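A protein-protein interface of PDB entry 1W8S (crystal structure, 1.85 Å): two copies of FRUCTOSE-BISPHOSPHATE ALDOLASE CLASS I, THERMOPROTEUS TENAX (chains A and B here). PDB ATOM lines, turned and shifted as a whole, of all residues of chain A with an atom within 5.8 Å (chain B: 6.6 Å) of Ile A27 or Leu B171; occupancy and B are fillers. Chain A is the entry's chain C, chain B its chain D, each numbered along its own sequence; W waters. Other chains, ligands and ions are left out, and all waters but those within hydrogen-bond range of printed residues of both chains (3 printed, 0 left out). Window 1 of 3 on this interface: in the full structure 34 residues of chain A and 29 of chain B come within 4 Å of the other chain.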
ATOM      1  N   ASP A  24      -0.735  18.337  -6.206  1.00  0.00           N
ATOM      2  CA  ASP A  24      -1.092  17.777  -7.522  1.00  0.00           C
ATOM      3  C   ASP A  24      -1.354  16.274  -7.487  1.00  0.00           C
ATOM      4  O   ASP A  24      -1.585  15.659  -8.519  1.00  0.00           O
ATOM      5  CB  ASP A  24      -0.066  18.147  -8.615  1.00  0.00           C
ATOM      6  CG  ASP A  24       1.321  17.700  -8.321  1.00  0.00           C
ATOM      7  OD1 ASP A  24       1.742  17.677  -7.150  1.00  0.00           O
ATOM      8  OD2 ASP A  24       2.104  17.351  -9.233  1.00  0.00           O
ATOM      9  N   HIS A  25      -1.424  15.708  -6.280  1.00  0.00           N
ATOM     10  CA  HIS A  25      -1.441  14.270  -6.088  1.00  0.00           C
ATOM     11  C   HIS A  25      -2.730  13.649  -6.598  1.00  0.00           C
ATOM     12  O   HIS A  25      -2.765  12.478  -6.967  1.00  0.00           O
ATOM     13  CB  HIS A  25      -1.256  13.964  -4.578  1.00  0.00           C
ATOM     14  CG  HIS A  25       0.050  14.470  -4.034  1.00  0.00           C
ATOM     15  ND1 HIS A  25       0.445  15.788  -4.154  1.00  0.00           N
ATOM     16  CD2 HIS A  25       1.051  13.837  -3.376  1.00  0.00           C
ATOM     17  CE1 HIS A  25       1.635  15.940  -3.605  1.00  0.00           C
ATOM     18  NE2 HIS A  25       2.028  14.770  -3.127  1.00  0.00           N
ATOM     19  N   GLY A  26      -3.799  14.421  -6.616  1.00  0.00           N
ATOM     20  CA  GLY A  26      -5.079  13.896  -7.020  1.00  0.00           C
ATOM     21  C   GLY A  26      -5.029  13.300  -8.413  1.00  0.00           C
ATOM     22  O   GLY A  26      -5.657  12.295  -8.668  1.00  0.00           O
ATOM     23  N   ILE A  27      -4.309  13.926  -9.326  1.00  0.00           N
ATOM     24  CA  ILE A  27      -4.084  13.296 -10.632  1.00  0.00           C
ATOM     25  C   ILE A  27      -2.864  12.332 -10.656  1.00  0.00           C
ATOM     26  O   ILE A  27      -2.993  11.194 -11.109  1.00  0.00           O
ATOM     27  CB  ILE A  27      -4.045  14.333 -11.774  1.00  0.00           C
ATOM     28  CG1 ILE A  27      -3.939  13.615 -13.140  1.00  0.00           C
ATOM     29  CG2 ILE A  27      -2.890  15.279 -11.613  1.00  0.00           C
ATOM     30  CD1 ILE A  27      -4.359  14.517 -14.374  1.00  0.00           C
ATOM     31  N   GLU A  28      -1.720  12.758 -10.115  1.00  0.00           N
ATOM     32  CA  GLU A  28      -0.476  11.978 -10.199  1.00  0.00           C
ATOM     33  C   GLU A  28      -0.583  10.609  -9.542  1.00  0.00           C
ATOM     34  O   GLU A  28      -0.113   9.624 -10.102  1.00  0.00           O
ATOM     35  CB  GLU A  28       0.708  12.747  -9.600  1.00  0.00           C
ATOM     36  CG  GLU A  28       1.102  13.986 -10.373  1.00  0.00           C
ATOM     37  CD  GLU A  28       1.694  13.676 -11.755  1.00  0.00           C
ATOM     38  OE1 GLU A  28       2.349  12.612 -11.926  1.00  0.00           O
ATOM     39  OE2 GLU A  28       1.488  14.487 -12.680  1.00  0.00           O
ATOM     40  N   HIS A  29      -1.205  10.556  -8.363  1.00  0.00           N
ATOM     41  CA  HIS A  29      -1.285   9.326  -7.553  1.00  0.00           C
ATOM     42  C   HIS A  29      -2.702   8.843  -7.319  1.00  0.00           C
ATOM     43  O   HIS A  29      -2.930   7.658  -7.064  1.00  0.00           O
ATOM     44  CB  HIS A  29      -0.647   9.522  -6.175  1.00  0.00           C
ATOM     45  CG  HIS A  29       0.792   9.919  -6.229  1.00  0.00           C
ATOM     46  ND1 HIS A  29       1.424  10.569  -5.188  1.00  0.00           N
ATOM     47  CD2 HIS A  29       1.727   9.763  -7.201  1.00  0.00           C
ATOM     48  CE1 HIS A  29       2.687  10.791  -5.516  1.00  0.00           C
ATOM     49  NE2 HIS A  29       2.893  10.318  -6.732  1.00  0.00           N
ATOM     50  N   GLY A  30      -3.657   9.754  -7.399  1.00  0.00           N
ATOM     51  CA  GLY A  30      -5.015   9.420  -7.118  1.00  0.00           C
ATOM     52  C   GLY A  30      -5.289   9.647  -5.649  1.00  0.00           C
ATOM     53  O   GLY A  30      -4.384   9.884  -4.855  1.00  0.00           O
ATOM     54  N   GLN A  61      -3.290  21.726  -9.732  1.00  0.00           N
ATOM     55  CA  GLN A  61      -3.690  21.523 -11.103  1.00  0.00           C
ATOM     56  C   GLN A  61      -4.788  22.527 -11.400  1.00  0.00           C
ATOM     57  O   GLN A  61      -5.404  23.084 -10.479  1.00  0.00           O
ATOM     58  CB  GLN A  61      -4.230  20.113 -11.295  1.00  0.00           C
ATOM     59  CG  GLN A  61      -3.225  19.020 -11.043  1.00  0.00           C
ATOM     60  CD  GLN A  61      -2.247  18.793 -12.179  1.00  0.00           C
ATOM     61  OE1 GLN A  61      -2.511  19.142 -13.321  1.00  0.00           O
ATOM     62  NE2 GLN A  61      -1.108  18.213 -11.851  1.00  0.00           N
ATOM     63  N   ARG A  62      -5.053  22.751 -12.682  1.00  0.00           N
ATOM     64  CA  ARG A  62      -6.024  23.752 -13.082  1.00  0.00           C
ATOM     65  C   ARG A  62      -7.431  23.594 -12.480  1.00  0.00           C
ATOM     66  O   ARG A  62      -8.084  24.575 -12.184  1.00  0.00           O
ATOM     67  CB  ARG A  62      -6.157  23.802 -14.600  1.00  0.00           C
ATOM     68  CG  ARG A  62      -6.798  22.551 -15.230  1.00  0.00           C
ATOM     69  CD  ARG A  62      -7.143  22.716 -16.706  1.00  0.00           C
ATOM     70  NE  ARG A  62      -7.893  23.946 -16.919  1.00  0.00           N
ATOM     71  CZ  ARG A  62      -7.884  24.631 -18.066  1.00  0.00           C
ATOM     72  NH1 ARG A  62      -7.207  24.208 -19.113  1.00  0.00           N
ATOM     73  NH2 ARG A  62      -8.566  25.748 -18.159  1.00  0.00           N
ATOM     74  N   GLY A  63      -7.912  22.378 -12.360  1.00  0.00           N
ATOM     75  CA  GLY A  63      -9.280  22.164 -11.912  1.00  0.00           C
ATOM     76  C   GLY A  63      -9.439  22.578 -10.468  1.00  0.00           C
ATOM     77  O   GLY A  63     -10.423  23.193 -10.096  1.00  0.00           O
ATOM     78  N   LYS A  78       0.309  23.868 -11.750  1.00  0.00           N
ATOM     79  CA  LYS A  78       1.018  22.735 -12.326  1.00  0.00           C
ATOM     80  C   LYS A  78       0.319  22.406 -13.631  1.00  0.00           C
ATOM     81  O   LYS A  78      -0.857  22.029 -13.650  1.00  0.00           O
ATOM     82  CB  LYS A  78       1.076  21.560 -11.327  1.00  0.00           C
ATOM     83  CG  LYS A  78       1.243  20.188 -11.904  1.00  0.00           C
ATOM     84  CD  LYS A  78       2.598  19.753 -12.306  1.00  0.00           C
ATOM     85  CE  LYS A  78       2.547  18.203 -12.714  1.00  0.00           C
ATOM     86  NZ  LYS A  78       1.481  17.335 -11.881  1.00  0.00           N
ATOM     87  N   ASN A  80       1.045  20.340 -16.397  1.00  0.00           N
ATOM     88  CA  ASN A  80       0.884  19.002 -16.951  1.00  0.00           C
ATOM     89  C   ASN A  80       0.419  18.003 -15.885  1.00  0.00           C
ATOM     90  O   ASN A  80       0.146  18.371 -14.755  1.00  0.00           O
ATOM     91  CB  ASN A  80       2.083  18.526 -17.783  1.00  0.00           C
ATOM     92  CG  ASN A  80       3.401  18.502 -17.062  1.00  0.00           C
ATOM     93  OD1 ASN A  80       3.557  19.012 -15.942  1.00  0.00           O
ATOM     94  ND2 ASN A  80       4.415  17.956 -17.753  1.00  0.00           N
ATOM     95  N   GLY A  81       0.286  16.748 -16.235  1.00  0.00           N
ATOM     96  CA  GLY A  81      -0.124  15.724 -15.282  1.00  0.00           C
ATOM     97  C   GLY A  81      -0.370  14.394 -15.962  1.00  0.00           C
ATOM     98  O   GLY A  81      -0.862  14.347 -17.093  1.00  0.00           O
ATOM     99  N   LYS A  82      -0.007  13.326 -15.268  1.00  0.00           N
ATOM    100  CA  LYS A  82      -0.211  11.956 -15.702  1.00  0.00           C
ATOM    101  C   LYS A  82      -0.701  11.156 -14.508  1.00  0.00           C
ATOM    102  O   LYS A  82      -0.695  11.679 -13.408  1.00  0.00           O
ATOM    103  CB  LYS A  82       1.066  11.336 -16.204  1.00  0.00           C
ATOM    104  CG  LYS A  82       2.202  11.132 -15.187  1.00  0.00           C
ATOM    105  CD  LYS A  82       3.228  10.182 -15.793  1.00  0.00           C
ATOM    106  CE  LYS A  82       3.927   9.306 -14.787  1.00  0.00           C
ATOM    107  NZ  LYS A  82       3.085   8.261 -14.085  1.00  0.00           N
ATOM    108  N   THR A  83      -1.121   9.911 -14.733  1.00  0.00           N
ATOM    109  CA  THR A  83      -1.607   9.058 -13.630  1.00  0.00           C
ATOM    110  C   THR A  83      -0.630   7.925 -13.436  1.00  0.00           C
ATOM    111  O   THR A  83       0.186   7.651 -14.322  1.00  0.00           O
ATOM    112  CB  THR A  83      -3.016   8.492 -13.902  1.00  0.00           C
ATOM    113  OG1 THR A  83      -2.992   7.532 -14.973  1.00  0.00           O
ATOM    114  CG2 THR A  83      -3.925   9.546 -14.383  1.00  0.00           C
ATOM    115  N   THR A  84      -0.693   7.281 -12.264  1.00  0.00           N
ATOM    116  CA  THR A  84       0.065   6.055 -12.005  1.00  0.00           C
ATOM    117  C   THR A  84      -0.560   4.809 -12.629  1.00  0.00           C
ATOM    118  O   THR A  84       0.068   3.751 -12.596  1.00  0.00           O
ATOM    119  CB  THR A  84       0.203   5.793 -10.478  1.00  0.00           C
ATOM    120  OG1 THR A  84      -1.092   5.832  -9.884  1.00  0.00           O
ATOM    121  CG2 THR A  84       0.917   6.906  -9.796  1.00  0.00           C
ATOM    122  N   ASN A  95      -2.284  20.172 -19.628  1.00  0.00           N
ATOM    123  CA  ASN A  95      -3.736  20.207 -19.676  1.00  0.00           C
ATOM    124  C   ASN A  95      -4.249  21.638 -19.510  1.00  0.00           C
ATOM    125  O   ASN A  95      -5.452  21.866 -19.458  1.00  0.00           O
ATOM    126  CB  ASN A  95      -4.323  19.277 -18.612  1.00  0.00           C
ATOM    127  CG  ASN A  95      -3.868  19.624 -17.218  1.00  0.00           C
ATOM    128  OD1 ASN A  95      -4.200  20.699 -16.718  1.00  0.00           O
ATOM    129  ND2 ASN A  95      -3.090  18.729 -16.583  1.00  0.00           N
ATOM    130  N   ILE B 113     -12.423  10.489 -21.275  1.00  0.00           N
ATOM    131  CA  ILE B 113     -11.002  10.202 -21.052  1.00  0.00           C
ATOM    132  C   ILE B 113     -10.864   8.763 -20.497  1.00  0.00           C
ATOM    133  O   ILE B 113     -11.786   8.262 -19.842  1.00  0.00           O
ATOM    134  CB  ILE B 113     -10.332  11.189 -20.091  1.00  0.00           C
ATOM    135  CG1 ILE B 113     -11.057  11.291 -18.730  1.00  0.00           C
ATOM    136  CG2 ILE B 113     -10.263  12.567 -20.707  1.00  0.00           C
ATOM    137  CD1 ILE B 113     -10.307  12.061 -17.680  1.00  0.00           C
ATOM    138  N   PHE B 124      -5.676  13.833 -22.752  1.00  0.00           N
ATOM    139  CA  PHE B 124      -5.428  14.983 -21.902  1.00  0.00           C
ATOM    140  C   PHE B 124      -5.029  16.229 -22.719  1.00  0.00           C
ATOM    141  O   PHE B 124      -5.466  17.341 -22.398  1.00  0.00           O
ATOM    142  CB  PHE B 124      -4.344  14.699 -20.850  1.00  0.00           C
ATOM    143  CG  PHE B 124      -4.722  13.647 -19.808  1.00  0.00           C
ATOM    144  CD1 PHE B 124      -6.023  13.146 -19.673  1.00  0.00           C
ATOM    145  CD2 PHE B 124      -3.753  13.147 -18.962  1.00  0.00           C
ATOM    146  CE1 PHE B 124      -6.327  12.204 -18.700  1.00  0.00           C
ATOM    147  CE2 PHE B 124      -4.045  12.210 -18.042  1.00  0.00           C
ATOM    148  CZ  PHE B 124      -5.354  11.716 -17.908  1.00  0.00           C
ATOM    149  N   LEU B 127      -8.218  17.422 -24.344  1.00  0.00           N
ATOM    150  CA  LEU B 127      -9.115  17.975 -23.371  1.00  0.00           C
ATOM    151  C   LEU B 127      -8.679  19.388 -23.012  1.00  0.00           C
ATOM    152  O   LEU B 127      -9.512  20.211 -22.707  1.00  0.00           O
ATOM    153  CB  LEU B 127      -9.140  17.125 -22.112  1.00  0.00           C
ATOM    154  CG  LEU B 127     -10.189  17.506 -21.060  1.00  0.00           C
ATOM    155  CD1 LEU B 127     -11.599  17.620 -21.679  1.00  0.00           C
ATOM    156  CD2 LEU B 127     -10.221  16.483 -19.916  1.00  0.00           C
ATOM    157  N   ALA B 128      -7.380  19.663 -23.031  1.00  0.00           N
ATOM    158  CA  ALA B 128      -6.902  20.979 -22.653  1.00  0.00           C
ATOM    159  C   ALA B 128      -7.516  22.011 -23.565  1.00  0.00           C
ATOM    160  O   ALA B 128      -7.896  23.099 -23.134  1.00  0.00           O
ATOM    161  CB  ALA B 128      -5.409  21.068 -22.770  1.00  0.00           C
ATOM    162  N   LYS B 131     -11.406  22.172 -22.958  1.00  0.00           N
ATOM    163  CA  LYS B 131     -11.689  22.906 -21.743  1.00  0.00           C
ATOM    164  C   LYS B 131     -11.594  24.402 -21.991  1.00  0.00           C
ATOM    165  O   LYS B 131     -12.446  25.195 -21.572  1.00  0.00           O
ATOM    166  CB  LYS B 131     -10.743  22.433 -20.606  1.00  0.00           C
ATOM    167  CG  LYS B 131     -10.693  23.315 -19.410  1.00  0.00           C
ATOM    168  CD  LYS B 131     -12.021  23.351 -18.628  1.00  0.00           C
ATOM    169  CE  LYS B 131     -11.955  24.230 -17.413  1.00  0.00           C
ATOM    170  NZ  LYS B 131     -13.275  24.280 -16.676  1.00  0.00           N
ATOM    171  N   LEU B 141     -18.473  21.743 -19.209  1.00  0.00           N
ATOM    172  CA  LEU B 141     -17.752  20.562 -19.685  1.00  0.00           C
ATOM    173  C   LEU B 141     -18.053  19.394 -18.760  1.00  0.00           C
ATOM    174  O   LEU B 141     -17.837  19.484 -17.567  1.00  0.00           O
ATOM    175  CB  LEU B 141     -16.251  20.823 -19.699  1.00  0.00           C
ATOM    176  CG  LEU B 141     -15.317  19.639 -19.938  1.00  0.00           C
ATOM    177  CD1 LEU B 141     -15.544  19.099 -21.358  1.00  0.00           C
ATOM    178  CD2 LEU B 141     -13.878  20.058 -19.726  1.00  0.00           C
ATOM    179  N   VAL B 143     -16.909  15.773 -18.014  1.00  0.00           N
ATOM    180  CA  VAL B 143     -15.855  14.827 -18.319  1.00  0.00           C
ATOM    181  C   VAL B 143     -16.396  13.462 -17.967  1.00  0.00           C
ATOM    182  O   VAL B 143     -16.882  13.242 -16.857  1.00  0.00           O
ATOM    183  CB  VAL B 143     -14.573  15.087 -17.562  1.00  0.00           C
ATOM    184  CG1 VAL B 143     -13.595  13.965 -17.811  1.00  0.00           C
ATOM    185  CG2 VAL B 143     -13.936  16.409 -18.026  1.00  0.00           C
ATOM    186  N   TYR B 163     -10.392   7.299  -8.357  1.00  0.00           N
ATOM    187  CA  TYR B 163      -9.327   7.921  -9.156  1.00  0.00           C
ATOM    188  C   TYR B 163      -9.982   8.629 -10.339  1.00  0.00           C
ATOM    189  O   TYR B 163      -9.652   9.781 -10.636  1.00  0.00           O
ATOM    190  CB  TYR B 163      -8.288   6.889  -9.597  1.00  0.00           C
ATOM    191  CG  TYR B 163      -6.866   7.388  -9.828  1.00  0.00           C
ATOM    192  CD1 TYR B 163      -5.793   6.517  -9.736  1.00  0.00           C
ATOM    193  CD2 TYR B 163      -6.594   8.711 -10.134  1.00  0.00           C
ATOM    194  CE1 TYR B 163      -4.492   6.957  -9.935  1.00  0.00           C
ATOM    195  CE2 TYR B 163      -5.310   9.153 -10.338  1.00  0.00           C
ATOM    196  CZ  TYR B 163      -4.263   8.283 -10.250  1.00  0.00           C
ATOM    197  OH  TYR B 163      -2.978   8.713 -10.459  1.00  0.00           O
ATOM    198  N   ARG B 166     -11.544  11.905  -9.204  1.00  0.00           N
ATOM    199  CA  ARG B 166     -10.585  12.929  -8.850  1.00  0.00           C
ATOM    200  C   ARG B 166      -9.917  13.541 -10.092  1.00  0.00           C
ATOM    201  O   ARG B 166      -9.718  14.748 -10.163  1.00  0.00           O
ATOM    202  CB  ARG B 166      -9.511  12.378  -7.932  1.00  0.00           C
ATOM    203  CG  ARG B 166      -8.615  13.444  -7.313  1.00  0.00           C
ATOM    204  CD  ARG B 166      -9.360  14.637  -6.696  1.00  0.00           C
ATOM    205  NE  ARG B 166      -8.439  15.567  -6.030  1.00  0.00           N
ATOM    206  CZ  ARG B 166      -8.674  16.141  -4.857  1.00  0.00           C
ATOM    207  NH1 ARG B 166      -9.797  15.875  -4.175  1.00  0.00           N
ATOM    208  NH2 ARG B 166      -7.763  16.937  -4.335  1.00  0.00           N
ATOM    209  N   ILE B 167      -9.574  12.701 -11.048  1.00  0.00           N
ATOM    210  CA  ILE B 167      -8.944  13.166 -12.278  1.00  0.00           C
ATOM    211  C   ILE B 167      -9.854  14.167 -13.005  1.00  0.00           C
ATOM    212  O   ILE B 167      -9.378  15.193 -13.521  1.00  0.00           O
ATOM    213  CB  ILE B 167      -8.596  11.983 -13.202  1.00  0.00           C
ATOM    214  CG1 ILE B 167      -7.478  11.135 -12.633  1.00  0.00           C
ATOM    215  CG2 ILE B 167      -8.122  12.493 -14.588  1.00  0.00           C
ATOM    216  CD1 ILE B 167      -7.460   9.743 -13.206  1.00  0.00           C
ATOM    217  N   ALA B 168     -11.149  13.864 -13.078  1.00  0.00           N
ATOM    218  CA  ALA B 168     -12.102  14.763 -13.691  1.00  0.00           C
ATOM    219  C   ALA B 168     -12.084  16.120 -13.028  1.00  0.00           C
ATOM    220  O   ALA B 168     -12.028  17.121 -13.719  1.00  0.00           O
ATOM    221  CB  ALA B 168     -13.493  14.189 -13.680  1.00  0.00           C
ATOM    222  N   LEU B 169     -12.092  16.157 -11.695  1.00  0.00           N
ATOM    223  CA  LEU B 169     -12.037  17.418 -10.965  1.00  0.00           C
ATOM    224  C   LEU B 169     -10.740  18.179 -11.314  1.00  0.00           C
ATOM    225  O   LEU B 169     -10.788  19.377 -11.659  1.00  0.00           O
ATOM    226  CB  LEU B 169     -12.143  17.163  -9.460  1.00  0.00           C
ATOM    227  CG  LEU B 169     -11.675  18.274  -8.515  1.00  0.00           C
ATOM    228  CD1 LEU B 169     -12.498  19.507  -8.668  1.00  0.00           C
ATOM    229  CD2 LEU B 169     -11.711  17.822  -7.054  1.00  0.00           C
ATOM    230  N   GLU B 170      -9.619  17.458 -11.290  1.00  0.00           N
ATOM    231  CA  GLU B 170      -8.281  18.034 -11.440  1.00  0.00           C
ATOM    232  C   GLU B 170      -8.048  18.685 -12.805  1.00  0.00           C
ATOM    233  O   GLU B 170      -7.374  19.700 -12.924  1.00  0.00           O
ATOM    234  CB  GLU B 170      -7.211  16.976 -11.206  1.00  0.00           C
ATOM    235  CG  GLU B 170      -7.162  16.331  -9.829  1.00  0.00           C
ATOM    236  CD  GLU B 170      -6.327  17.073  -8.798  1.00  0.00           C
ATOM    237  OE1 GLU B 170      -5.442  17.885  -9.162  1.00  0.00           O
ATOM    238  OE2 GLU B 170      -6.528  16.819  -7.580  1.00  0.00           O
ATOM    239  N   LEU B 171      -8.637  18.098 -13.828  1.00  0.00           N
ATOM    240  CA  LEU B 171      -8.450  18.527 -15.192  1.00  0.00           C
ATOM    241  C   LEU B 171      -9.445  19.617 -15.602  1.00  0.00           C
ATOM    242  O   LEU B 171      -9.319  20.133 -16.700  1.00  0.00           O
ATOM    243  CB  LEU B 171      -8.614  17.321 -16.118  1.00  0.00           C
ATOM    244  CG  LEU B 171      -7.517  16.271 -15.983  1.00  0.00           C
ATOM    245  CD1 LEU B 171      -7.815  15.130 -16.932  1.00  0.00           C
ATOM    246  CD2 LEU B 171      -6.141  16.831 -16.257  1.00  0.00           C
ATOM    247  N   GLY B 172     -10.454  19.891 -14.778  1.00  0.00           N
ATOM    248  CA  GLY B 172     -11.333  21.053 -14.967  1.00  0.00           C
ATOM    249  C   GLY B 172     -12.802  20.776 -15.315  1.00  0.00           C
ATOM    250  O   GLY B 172     -13.533  21.666 -15.754  1.00  0.00           O
ATOM    251  N   ALA B 173     -13.232  19.538 -15.130  1.00  0.00           N
ATOM    252  CA  ALA B 173     -14.622  19.169 -15.332  1.00  0.00           C
ATOM    253  C   ALA B 173     -15.560  20.088 -14.542  1.00  0.00           C
ATOM    254  O   ALA B 173     -15.282  20.436 -13.411  1.00  0.00           O
ATOM    255  CB  ALA B 173     -14.836  17.729 -14.907  1.00  0.00           C
HETATM  256  O   HOH W   1      -4.254  19.917  -7.731  1.00  0.00           O
HETATM  257  O   HOH W   2      -7.853  20.075 -19.140  1.00  0.00           O
HETATM  258  O   HOH W   3      -4.925  16.979  -5.544  1.00  0.00           O
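The side-chain hydroxyl (OH) of Tyr B163 sits close to the backbone NH (N) of Gly A30 (3.3 Å). OH of Tyr B163 sits close to N of His A29 (3.3 Å). O of Ile A27 sits at hydrogen-bond distance from OH of Tyr B163 (2.6 Å). The side-chain hydroxyl (OH) of Tyr B163 lies within hydrogen-bond range of the backbone NH (N) of Thr A84, at 3.2 Å. O of Glu A28 is in hydrogen-bond range of OH of Tyr B163, at 3.0 Å. The backbone NH (N) of Gly A63 sits at hydrogen-bond distance from the backbone carbonyl oxygen (O) of Glu B170 (2.8 Å).
Among the printed residues, merely in contact across the chains: Gln A61 with Glu B170, Gly A63 with Leu B169, Gly A26 with Glu B170, Arg A62 with Leu B171, Arg A62 with Lys B131, Asn A95 with Ala B128, Thr A83 with Tyr B163, Gly A26 with Arg B166, Ile A27 with Leu B171, Gly A26 with Tyr B163, Asn A95 with Leu B171, Gly A81 with Phe B124, Arg A62 with Glu B170, Thr A83 with Ile B167, Ile A27 with Glu B170 and Gly A63 with Gly B172.
No position is printed for both chains. Of the 22 pairs that touch across the chains among the printed residues, none has its exchanged pair printed and touching as well.
Of the 17 printed residues of chain A, 12 touch a printed residue of chain B. Printed residues of chain A that touch a printed residue of chain B: Gly A26, Ile A27, Glu A28, His A29, Gly A30, Gln A61, Arg A62, Gly A63, Gly A81, Thr A83, Thr A84 and Asn A95. Hydrophobic or aromatic side chains of chain A that line the printed part of chain B: Ile A27. Among the printed residues, no Asp or Glu carboxylate lies within 4 Å of a Lys or Arg side-chain nitrogen of the other chain.
Water W3 lies within hydrogen-bond range of the side-chain carboxylate of Glu B170 (2.6 Å), the backbone NH of Gly A26 (3.0 Å) and the guanidinium group of Arg B166 (3.1 Å). Water W1 lies within hydrogen-bond range of OE1 of Glu B170 and N of Gln A61. Water W2 bridges O of Leu B171 (2.8 Å) and O of Asn A95 (3.0 Å).
His A25 touches none of the printed residues of chain B. Printed residues of chain B within 4 Å of Ile A27: Tyr B163 (2.6 Å), Glu B170 (3.8 Å) and Leu B171 (3.5 Å). Of the printed residues of chain B, Arg A62 touches Lys B131 (3.4 Å), Glu B170 (3.7 Å) and Leu B171 (3.4 Å). Leu B141 touches none of the printed residues of chain A. Of the printed residues of chain A, Leu B171 touches Ile A27 (3.5 Å), Arg A62 (3.4 Å) and Asn A95 (3.6 Å). Of the printed residues of chain A, Gly B172 touches Gly A63 (3.8 Å). The nearest residue of chain B that does not touch Ile A27 is Ile B167 (4.3 Å).
The guanidinium group (NE) of Arg B166 is in salt-bridge range of the side-chain carboxylate (OE2) of Glu B170, at 2.8 Å. The guanidinium group (NH1) of Arg A62 sits at hydrogen-bond distance from the backbone carbonyl oxygen (O) of Asn A95 (2.9 Å). The side-chain amide nitrogen (NE2) of Gln A61 lies close to the side-chain amino group (NZ) of Lys A78, at 2.7 Å. The backbone carbonyl oxygen (O) of Glu A28 lies close to the backbone NH (N) of Thr A84 (3.2 Å). OE2 of Glu A28 lies within salt-bridge range of NZ of Lys A78 (3.0 Å). NZ of Lys B131 is in hydrogen-bond range of O of Gly B172 (2.8 Å).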
